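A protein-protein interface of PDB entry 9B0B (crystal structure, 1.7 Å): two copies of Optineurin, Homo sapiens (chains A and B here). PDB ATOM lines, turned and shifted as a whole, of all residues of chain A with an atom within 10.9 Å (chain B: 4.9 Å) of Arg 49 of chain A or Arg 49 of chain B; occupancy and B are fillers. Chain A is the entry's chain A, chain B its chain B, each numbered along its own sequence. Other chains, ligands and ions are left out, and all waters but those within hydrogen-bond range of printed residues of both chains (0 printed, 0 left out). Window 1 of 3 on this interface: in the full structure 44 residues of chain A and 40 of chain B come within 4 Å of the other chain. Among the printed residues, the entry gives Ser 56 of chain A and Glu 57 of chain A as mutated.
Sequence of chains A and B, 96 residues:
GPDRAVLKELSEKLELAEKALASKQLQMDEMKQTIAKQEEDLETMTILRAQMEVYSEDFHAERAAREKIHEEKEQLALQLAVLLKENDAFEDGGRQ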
ATOM      1  N   ASP A  41     -23.549   4.962  32.269  1.00  0.00           N
ATOM      2  CA  ASP A  41     -22.417   5.881  32.271  1.00  0.00           C
ATOM      3  C   ASP A  41     -22.363   6.717  31.001  1.00  0.00           C
ATOM      4  O   ASP A  41     -22.012   7.904  31.047  1.00  0.00           O
ATOM      5  CB  ASP A  41     -21.098   5.117  32.454  1.00  0.00           C
ATOM      6  CG  ASP A  41     -20.982   4.462  33.826  1.00  0.00           C
ATOM      7  OD1 ASP A  41     -21.778   4.811  34.732  1.00  0.00           O
ATOM      8  OD2 ASP A  41     -20.076   3.615  33.998  1.00  0.00           O
ATOM      9  N   LEU A  42     -22.680   6.120  29.859  1.00  0.00           N
ATOM     10  CA  LEU A  42     -22.607   6.885  28.618  1.00  0.00           C
ATOM     11  C   LEU A  42     -23.709   7.936  28.560  1.00  0.00           C
ATOM     12  O   LEU A  42     -23.481   9.068  28.093  1.00  0.00           O
ATOM     13  CB  LEU A  42     -22.677   5.950  27.412  1.00  0.00           C
ATOM     14  CG  LEU A  42     -22.570   6.530  25.992  1.00  0.00           C
ATOM     15  CD1 LEU A  42     -21.287   7.349  25.768  1.00  0.00           C
ATOM     16  CD2 LEU A  42     -22.638   5.412  24.970  1.00  0.00           C
ATOM     17  N   GLU A  43     -24.919   7.583  29.018  1.00  0.00           N
ATOM     18  CA  GLU A  43     -25.976   8.580  29.019  1.00  0.00           C
ATOM     19  C   GLU A  43     -25.610   9.753  29.927  1.00  0.00           C
ATOM     20  O   GLU A  43     -25.764  10.923  29.535  1.00  0.00           O
ATOM     21  CB  GLU A  43     -27.313   7.947  29.424  1.00  0.00           C
ATOM     22  CG  GLU A  43     -28.480   8.794  28.905  1.00  0.00           C
ATOM     23  CD  GLU A  43     -29.819   8.438  29.518  1.00  0.00           C
ATOM     24  OE1 GLU A  43     -30.099   7.226  29.659  1.00  0.00           O
ATOM     25  OE2 GLU A  43     -30.587   9.372  29.853  1.00  0.00           O
ATOM     26  N   THR A  44     -25.082   9.467  31.122  1.00  0.00           N
ATOM     27  CA  THR A  44     -24.621  10.531  32.010  1.00  0.00           C
ATOM     28  C   THR A  44     -23.585  11.435  31.333  1.00  0.00           C
ATOM     29  O   THR A  44     -23.736  12.663  31.296  1.00  0.00           O
ATOM     30  CB  THR A  44     -24.027   9.941  33.289  1.00  0.00           C
ATOM     31  OG1 THR A  44     -25.043   9.214  33.973  1.00  0.00           O
ATOM     32  CG2 THR A  44     -23.576  11.071  34.196  1.00  0.00           C
ATOM     33  N   MET A  45     -22.511  10.847  30.820  1.00  0.00           N
ATOM     34  CA  MET A  45     -21.447  11.624  30.194  1.00  0.00           C
ATOM     35  C   MET A  45     -21.975  12.432  29.011  1.00  0.00           C
ATOM     36  O   MET A  45     -21.503  13.555  28.743  1.00  0.00           O
ATOM     37  CB  MET A  45     -20.327  10.666  29.747  1.00  0.00           C
ATOM     38  CG  MET A  45     -18.954  11.327  29.610  1.00  0.00           C
ATOM     39  SD  MET A  45     -18.417  12.124  31.163  1.00  0.00           S
ATOM     40  CE  MET A  45     -17.898  10.717  32.136  1.00  0.00           C
ATOM     41  N   THR A  46     -22.951  11.871  28.286  1.00  0.00           N
ATOM     42  CA  THR A  46     -23.501  12.557  27.120  1.00  0.00           C
ATOM     43  C   THR A  46     -24.239  13.824  27.537  1.00  0.00           C
ATOM     44  O   THR A  46     -24.054  14.897  26.931  1.00  0.00           O
ATOM     45  CB  THR A  46     -24.425  11.616  26.338  1.00  0.00           C
ATOM     46  OG1 THR A  46     -23.634  10.523  25.837  1.00  0.00           O
ATOM     47  CG2 THR A  46     -25.039  12.363  25.149  1.00  0.00           C
ATOM     48  N   ILE A  47     -25.068  13.714  28.583  1.00  0.00           N
ATOM     49  CA  ILE A  47     -25.771  14.874  29.129  1.00  0.00           C
ATOM     50  C   ILE A  47     -24.773  15.914  29.624  1.00  0.00           C
ATOM     51  O   ILE A  47     -24.922  17.128  29.381  1.00  0.00           O
ATOM     52  CB  ILE A  47     -26.699  14.457  30.280  1.00  0.00           C
ATOM     53  CG1 ILE A  47     -27.766  13.468  29.824  1.00  0.00           C
ATOM     54  CG2 ILE A  47     -27.378  15.688  30.902  1.00  0.00           C
ATOM     55  CD1 ILE A  47     -28.567  12.968  30.978  1.00  0.00           C
ATOM     56  N   LEU A  48     -23.755  15.451  30.357  1.00  0.00           N
ATOM     57  CA  LEU A  48     -22.816  16.398  30.947  1.00  0.00           C
ATOM     58  C   LEU A  48     -22.087  17.184  29.869  1.00  0.00           C
ATOM     59  O   LEU A  48     -21.901  18.406  29.997  1.00  0.00           O
ATOM     60  CB  LEU A  48     -21.812  15.661  31.824  1.00  0.00           C
ATOM     61  CG  LEU A  48     -22.390  15.136  33.141  1.00  0.00           C
ATOM     62  CD1 LEU A  48     -21.259  14.362  33.894  1.00  0.00           C
ATOM     63  CD2 LEU A  48     -22.996  16.223  33.978  1.00  0.00           C
ATOM     64  N   ARG A  49     -21.650  16.496  28.809  1.00  0.00           N
ATOM     65  CA  ARG A  49     -20.978  17.182  27.707  1.00  0.00           C
ATOM     66  C   ARG A  49     -21.908  18.200  27.048  1.00  0.00           C
ATOM     67  O   ARG A  49     -21.506  19.337  26.742  1.00  0.00           O
ATOM     68  CB  ARG A  49     -20.510  16.177  26.648  1.00  0.00           C
ATOM     69  CG  ARG A  49     -19.607  16.853  25.617  1.00  0.00           C
ATOM     70  CD  ARG A  49     -19.763  16.260  24.224  1.00  0.00           C
ATOM     71  NE  ARG A  49     -21.114  16.514  23.735  1.00  0.00           N
ATOM     72  CZ  ARG A  49     -21.466  17.585  23.020  1.00  0.00           C
ATOM     73  NH1 ARG A  49     -20.552  18.497  22.681  1.00  0.00           N
ATOM     74  NH2 ARG A  49     -22.740  17.744  22.643  1.00  0.00           N
ATOM     75  N   ALA A  50     -23.158  17.802  26.801  1.00  0.00           N
ATOM     76  CA  ALA A  50     -24.089  18.711  26.146  1.00  0.00           C
ATOM     77  C   ALA A  50     -24.331  19.969  26.967  1.00  0.00           C
ATOM     78  O   ALA A  50     -24.446  21.083  26.407  1.00  0.00           O
ATOM     79  CB  ALA A  50     -25.423  17.991  25.888  1.00  0.00           C
ATOM     80  N   GLN A  51     -24.494  19.821  28.284  1.00  0.00           N
ATOM     81  CA  GLN A  51     -24.772  21.011  29.094  1.00  0.00           C
ATOM     82  C   GLN A  51     -23.588  21.961  29.128  1.00  0.00           C
ATOM     83  O   GLN A  51     -23.758  23.159  29.406  1.00  0.00           O
ATOM     84  CB  GLN A  51     -25.119  20.625  30.522  1.00  0.00           C
ATOM     85  CG  GLN A  51     -26.388  19.795  30.712  1.00  0.00           C
ATOM     86  CD  GLN A  51     -26.536  19.390  32.169  1.00  0.00           C
ATOM     87  OE1 GLN A  51     -25.553  19.408  32.932  1.00  0.00           O
ATOM     88  NE2 GLN A  51     -27.743  19.028  32.567  1.00  0.00           N
ATOM     89  N   MET A  52     -22.393  21.462  28.875  1.00  0.00           N
ATOM     90  CA  MET A  52     -21.166  22.255  28.934  1.00  0.00           C
ATOM     91  C   MET A  52     -20.730  22.795  27.578  1.00  0.00           C
ATOM     92  O   MET A  52     -19.791  23.583  27.518  1.00  0.00           O
ATOM     93  CB  MET A  52     -20.047  21.381  29.515  1.00  0.00           C
ATOM     94  CG  MET A  52     -20.343  20.936  30.937  1.00  0.00           C
ATOM     95  SD  MET A  52     -19.888  22.262  32.068  1.00  0.00           S
ATOM     96  CE  MET A  52     -18.086  22.176  32.023  1.00  0.00           C
ATOM     97  N   GLU A  53     -21.387  22.370  26.495  1.00  0.00           N
ATOM     98  CA  GLU A  53     -20.979  22.718  25.139  1.00  0.00           C
ATOM     99  C   GLU A  53     -20.898  24.234  24.920  1.00  0.00           C
ATOM    100  O   GLU A  53     -20.013  24.712  24.194  1.00  0.00           O
ATOM    101  CB  GLU A  53     -21.986  22.065  24.178  1.00  0.00           C
ATOM    102  CG  GLU A  53     -21.698  22.318  22.725  1.00  0.00           C
ATOM    103  CD  GLU A  53     -22.667  21.579  21.804  1.00  0.00           C
ATOM    104  OE1 GLU A  53     -23.697  22.172  21.401  1.00  0.00           O
ATOM    105  OE2 GLU A  53     -22.402  20.396  21.503  1.00  0.00           O
ATOM    106  N   VAL A  54     -21.782  25.002  25.566  1.00  0.00           N
ATOM    107  CA  VAL A  54     -21.789  26.463  25.445  1.00  0.00           C
ATOM    108  C   VAL A  54     -20.407  27.063  25.711  1.00  0.00           C
ATOM    109  O   VAL A  54     -20.061  28.139  25.187  1.00  0.00           O
ATOM    110  CB  VAL A  54     -22.836  27.077  26.407  1.00  0.00           C
ATOM    111  CG1 VAL A  54     -22.607  26.652  27.851  1.00  0.00           C
ATOM    112  CG2 VAL A  54     -22.719  28.507  26.381  1.00  0.00           C
ATOM    113  N   TYR A  55     -19.639  26.447  26.616  1.00  0.00           N
ATOM    114  CA  TYR A  55     -18.378  27.071  27.010  1.00  0.00           C
ATOM    115  C   TYR A  55     -17.380  27.149  25.864  1.00  0.00           C
ATOM    116  O   TYR A  55     -16.466  27.975  25.916  1.00  0.00           O
ATOM    117  CB  TYR A  55     -17.811  26.313  28.216  1.00  0.00           C
ATOM    118  CG  TYR A  55     -18.585  26.620  29.488  1.00  0.00           C
ATOM    119  CD1 TYR A  55     -18.674  27.913  29.967  1.00  0.00           C
ATOM    120  CD2 TYR A  55     -19.319  25.633  30.154  1.00  0.00           C
ATOM    121  CE1 TYR A  55     -19.386  28.200  31.101  1.00  0.00           C
ATOM    122  CE2 TYR A  55     -20.068  25.929  31.306  1.00  0.00           C
ATOM    123  CZ  TYR A  55     -20.092  27.196  31.769  1.00  0.00           C
ATOM    124  OH  TYR A  55     -20.791  27.524  32.903  1.00  0.00           O
ATOM    125  N   SER A  56     -17.458  26.275  24.854  1.00  0.00           N
ATOM    126  CA  SER A  56     -16.566  26.459  23.711  1.00  0.00           C
ATOM    127  C   SER A  56     -16.865  27.783  23.025  1.00  0.00           C
ATOM    128  O   SER A  56     -15.954  28.572  22.729  1.00  0.00           O
ATOM    129  CB  SER A  56     -16.690  25.306  22.706  1.00  0.00           C
ATOM    130  OG  SER A  56     -15.959  25.632  21.518  1.00  0.00           O
ATOM    131  N   GLU A  57     -18.147  28.060  22.797  1.00  0.00           N
ATOM    132  CA  GLU A  57     -18.501  29.325  22.172  1.00  0.00           C
ATOM    133  C   GLU A  57     -18.118  30.500  23.058  1.00  0.00           C
ATOM    134  O   GLU A  57     -17.547  31.490  22.581  1.00  0.00           O
ATOM    135  CB  GLU A  57     -19.997  29.367  21.871  1.00  0.00           C
ATOM    136  CG  GLU A  57     -20.478  30.736  21.379  1.00  0.00           C
ATOM    137  CD  GLU A  57     -21.887  30.680  20.732  1.00  0.00           C
ATOM    138  OE1 GLU A  57     -22.652  29.719  20.994  1.00  0.00           O
ATOM    139  OE2 GLU A  57     -22.191  31.579  19.915  1.00  0.00           O
ATOM    140  N   MET B  45     -16.698  10.256  24.733  1.00  0.00           N
ATOM    141  CA  MET B  45     -17.535  11.231  25.428  1.00  0.00           C
ATOM    142  C   MET B  45     -16.851  11.775  26.671  1.00  0.00           C
ATOM    143  O   MET B  45     -17.047  12.951  27.046  1.00  0.00           O
ATOM    144  CB  MET B  45     -18.881  10.571  25.801  1.00  0.00           C
ATOM    145  CG  MET B  45     -19.958  11.582  26.154  1.00  0.00           C
ATOM    146  SD  MET B  45     -20.360  12.699  24.750  1.00  0.00           S
ATOM    147  CE  MET B  45     -21.129  11.520  23.593  1.00  0.00           C
ATOM    148  N   THR B  46     -16.085  10.940  27.360  1.00  0.00           N
ATOM    149  CA  THR B  46     -15.434  11.405  28.562  1.00  0.00           C
ATOM    150  C   THR B  46     -14.387  12.448  28.206  1.00  0.00           C
ATOM    151  O   THR B  46     -14.171  13.396  28.962  1.00  0.00           O
ATOM    152  CB  THR B  46     -14.759  10.228  29.265  1.00  0.00           C
ATOM    153  OG1 THR B  46     -15.796   9.342  29.705  1.00  0.00           O
ATOM    154  CG2 THR B  46     -13.943  10.708  30.459  1.00  0.00           C
ATOM    155  N   ILE B  47     -13.685  12.231  27.090  1.00  0.00           N
ATOM    156  CA  ILE B  47     -12.669  13.217  26.706  1.00  0.00           C
ATOM    157  C   ILE B  47     -13.356  14.497  26.248  1.00  0.00           C
ATOM    158  O   ILE B  47     -12.883  15.595  26.538  1.00  0.00           O
ATOM    159  CB  ILE B  47     -11.751  12.640  25.618  1.00  0.00           C
ATOM    160  CG1 ILE B  47     -10.801  11.590  26.234  1.00  0.00           C
ATOM    161  CG2 ILE B  47     -10.920  13.767  24.953  1.00  0.00           C
ATOM    162  CD1 ILE B  47     -10.271  10.643  25.194  1.00  0.00           C
ATOM    163  N   LEU B  48     -14.464  14.369  25.496  1.00  0.00           N
ATOM    164  CA  LEU B  48     -15.169  15.559  25.006  1.00  0.00           C
ATOM    165  C   LEU B  48     -15.726  16.344  26.176  1.00  0.00           C
ATOM    166  O   LEU B  48     -15.671  17.581  26.197  1.00  0.00           O
ATOM    167  CB  LEU B  48     -16.290  15.155  24.048  1.00  0.00           C
ATOM    168  CG  LEU B  48     -15.768  14.613  22.705  1.00  0.00           C
ATOM    169  CD1 LEU B  48     -16.910  14.156  21.808  1.00  0.00           C
ATOM    170  CD2 LEU B  48     -14.777  15.610  22.028  1.00  0.00           C
ATOM    171  N   ARG B  49     -16.296  15.647  27.181  1.00  0.00           N
ATOM    172  CA  ARG B  49     -16.727  16.394  28.366  1.00  0.00           C
ATOM    173  C   ARG B  49     -15.540  17.108  29.021  1.00  0.00           C
ATOM    174  O   ARG B  49     -15.627  18.286  29.444  1.00  0.00           O
ATOM    175  CB  ARG B  49     -17.393  15.454  29.381  1.00  0.00           C
ATOM    176  CG  ARG B  49     -18.122  16.313  30.446  1.00  0.00           C
ATOM    177  CD  ARG B  49     -18.026  15.798  31.898  1.00  0.00           C
ATOM    178  NE  ARG B  49     -16.655  15.818  32.382  1.00  0.00           N
ATOM    179  CZ  ARG B  49     -16.127  16.816  33.110  1.00  0.00           C
ATOM    180  NH1 ARG B  49     -16.858  17.864  33.464  1.00  0.00           N
ATOM    181  NH2 ARG B  49     -14.855  16.762  33.493  1.00  0.00           N
ATOM    182  N   ALA B  50     -14.402  16.417  29.123  1.00  0.00           N
ATOM    183  CA  ALA B  50     -13.226  17.052  29.705  1.00  0.00           C
ATOM    184  C   ALA B  50     -12.806  18.259  28.880  1.00  0.00           C
ATOM    185  O   ALA B  50     -12.409  19.297  29.439  1.00  0.00           O
ATOM    186  CB  ALA B  50     -12.063  16.061  29.813  1.00  0.00           C
ATOM    187  N   GLN B  51     -12.901  18.144  27.554  1.00  0.00           N
ATOM    188  CA  GLN B  51     -12.559  19.284  26.692  1.00  0.00           C
ATOM    189  C   GLN B  51     -13.473  20.470  26.988  1.00  0.00           C
ATOM    190  O   GLN B  51     -13.002  21.613  27.070  1.00  0.00           O
ATOM    191  CB  GLN B  51     -12.699  18.877  25.216  1.00  0.00           C
ATOM    192  CG  GLN B  51     -12.300  20.068  24.287  1.00  0.00           C
ATOM    193  CD  GLN B  51     -12.577  19.797  22.838  1.00  0.00           C
ATOM    194  OE1 GLN B  51     -13.310  18.873  22.504  1.00  0.00           O
ATOM    195  NE2 GLN B  51     -11.930  20.541  21.959  1.00  0.00           N
ATOM    196  N   MET B  52     -14.783  20.226  27.207  1.00  0.00           N
ATOM    197  CA  MET B  52     -15.674  21.354  27.549  1.00  0.00           C
ATOM    198  C   MET B  52     -15.321  21.936  28.897  1.00  0.00           C
ATOM    199  O   MET B  52     -15.448  23.153  29.112  1.00  0.00           O
ATOM    200  CB  MET B  52     -17.150  20.936  27.481  1.00  0.00           C
ATOM    201  CG  MET B  52     -17.294  20.302  26.117  1.00  0.00           C
ATOM    202  SD  MET B  52     -17.393  21.502  24.756  1.00  0.00           S
ATOM    203  CE  MET B  52     -16.033  22.151  24.129  1.00  0.00           C
ATOM    204  N   GLU B  53     -14.859  21.092  29.815  1.00  0.00           N
ATOM    205  CA  GLU B  53     -14.419  21.605  31.100  1.00  0.00           C
ATOM    206  C   GLU B  53     -13.173  22.473  30.940  1.00  0.00           C
ATOM    207  O   GLU B  53     -13.046  23.496  31.618  1.00  0.00           O
ATOM    208  CB  GLU B  53     -14.162  20.459  32.088  1.00  0.00           C
ATOM    209  CG  GLU B  53     -13.707  20.940  33.494  1.00  0.00           C
ATOM    210  CD  GLU B  53     -14.035  19.952  34.623  1.00  0.00           C
ATOM    211  OE1 GLU B  53     -14.219  18.748  34.334  1.00  0.00           O
ATOM    212  OE2 GLU B  53     -14.099  20.385  35.800  1.00  0.00           O
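The backbone carbonyl oxygen (O) of Leu 42 of chain A is in hydrogen-bond range of the side-chain hydroxyl (OG1) of Thr 46 of chain A (2.7 Å).
NH1 of Arg 49 of chain A lies within salt-bridge range of OE2 of Glu 53 of chain A (2.9 Å).
The side-chain carboxylate (OE1) of Glu 53 of chain B is in salt-bridge range of the guanidinium group (NH1) of Arg 49 of chain B.
Among the printed residues, pairs that only touch across the chains: Met 45 of chain A with Met 45 of chain B, Met 45 of chain A with Thr 46 of chain B, Met 45 of chain A with Arg 49 of chain B, Thr 46 of chain A with Met 45 of chain B, Leu 48 of chain A with Arg 49 of chain B, Arg 49 of chain A with Met 45 of chain B, Arg 49 of chain A with Leu 48 of chain B, Arg 49 of chain A with Arg 49 of chain B, Met 52 of chain A with Met 52 of chain B, Met 52 of chain A with Glu 53 of chain B, Glu 53 of chain A with Met 52 of chain B and Ser 56 of chain A with Met 52 of chain B.
Printed residues of chain B within 4 Å of Arg 49 of chain A: Met 45, Leu 48 and Arg 49.
Leu 48 of chain B touches one residue of chain A.
No residue of chain A comes within 4 Å of Ala 50 of chain B.
Of the printed residues of chain B, Thr 46 of chain A touches Met 45 (3.5 Å).
Printed residues of chain A within 4 Å of Glu 53 of chain B: Met 52 (3.8 Å).
Of the printed residues of chain B, Ser 56 of chain A touches Met 52.
Ile 47 of chain B touches none of the printed residues of chain A.
The nearest printed residue of chain B that does not touch Arg 49 of chain A is Met 52 of chain B (4.2 Å).
The nearest printed residue of chain A that does not touch Arg 49 of chain B is Met 52 of chain A (4.7 Å).
The nearest printed residue of chain A that does not touch Met 45 of chain B is Leu 42 of chain A (4.02 Å).
Hydrophobic or aromatic side chains of chain A within 4 Å of the printed part of chain B: Met 45, Leu 48 and Met 52.
Of the 9 printed residues of chain B, 6 touch a printed residue of chain A.
Met 45 of chain A touches Thr 46 of chain B, and with the chains exchanged Thr 46 of chain A touches Met 45 of chain B.
Met 45 of chain A touches Arg 49 of chain B, and with the chains exchanged Arg 49 of chain A touches Met 45 of chain B.
Leu 48 of chain A touches Arg 49 of chain B, and with the chains exchanged Arg 49 of chain A touches Leu 48 of chain B.
Arg 49 of chain A touches its own counterpart, Arg 49 of chain B.
Positions printed for both chains: 45, 46, 47, 48, 49, 50, 51, 52 and 53.
Of the 12 pairs that touch across the chains among the printed residues, 11 have their exchanged pair printed and touching as well.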
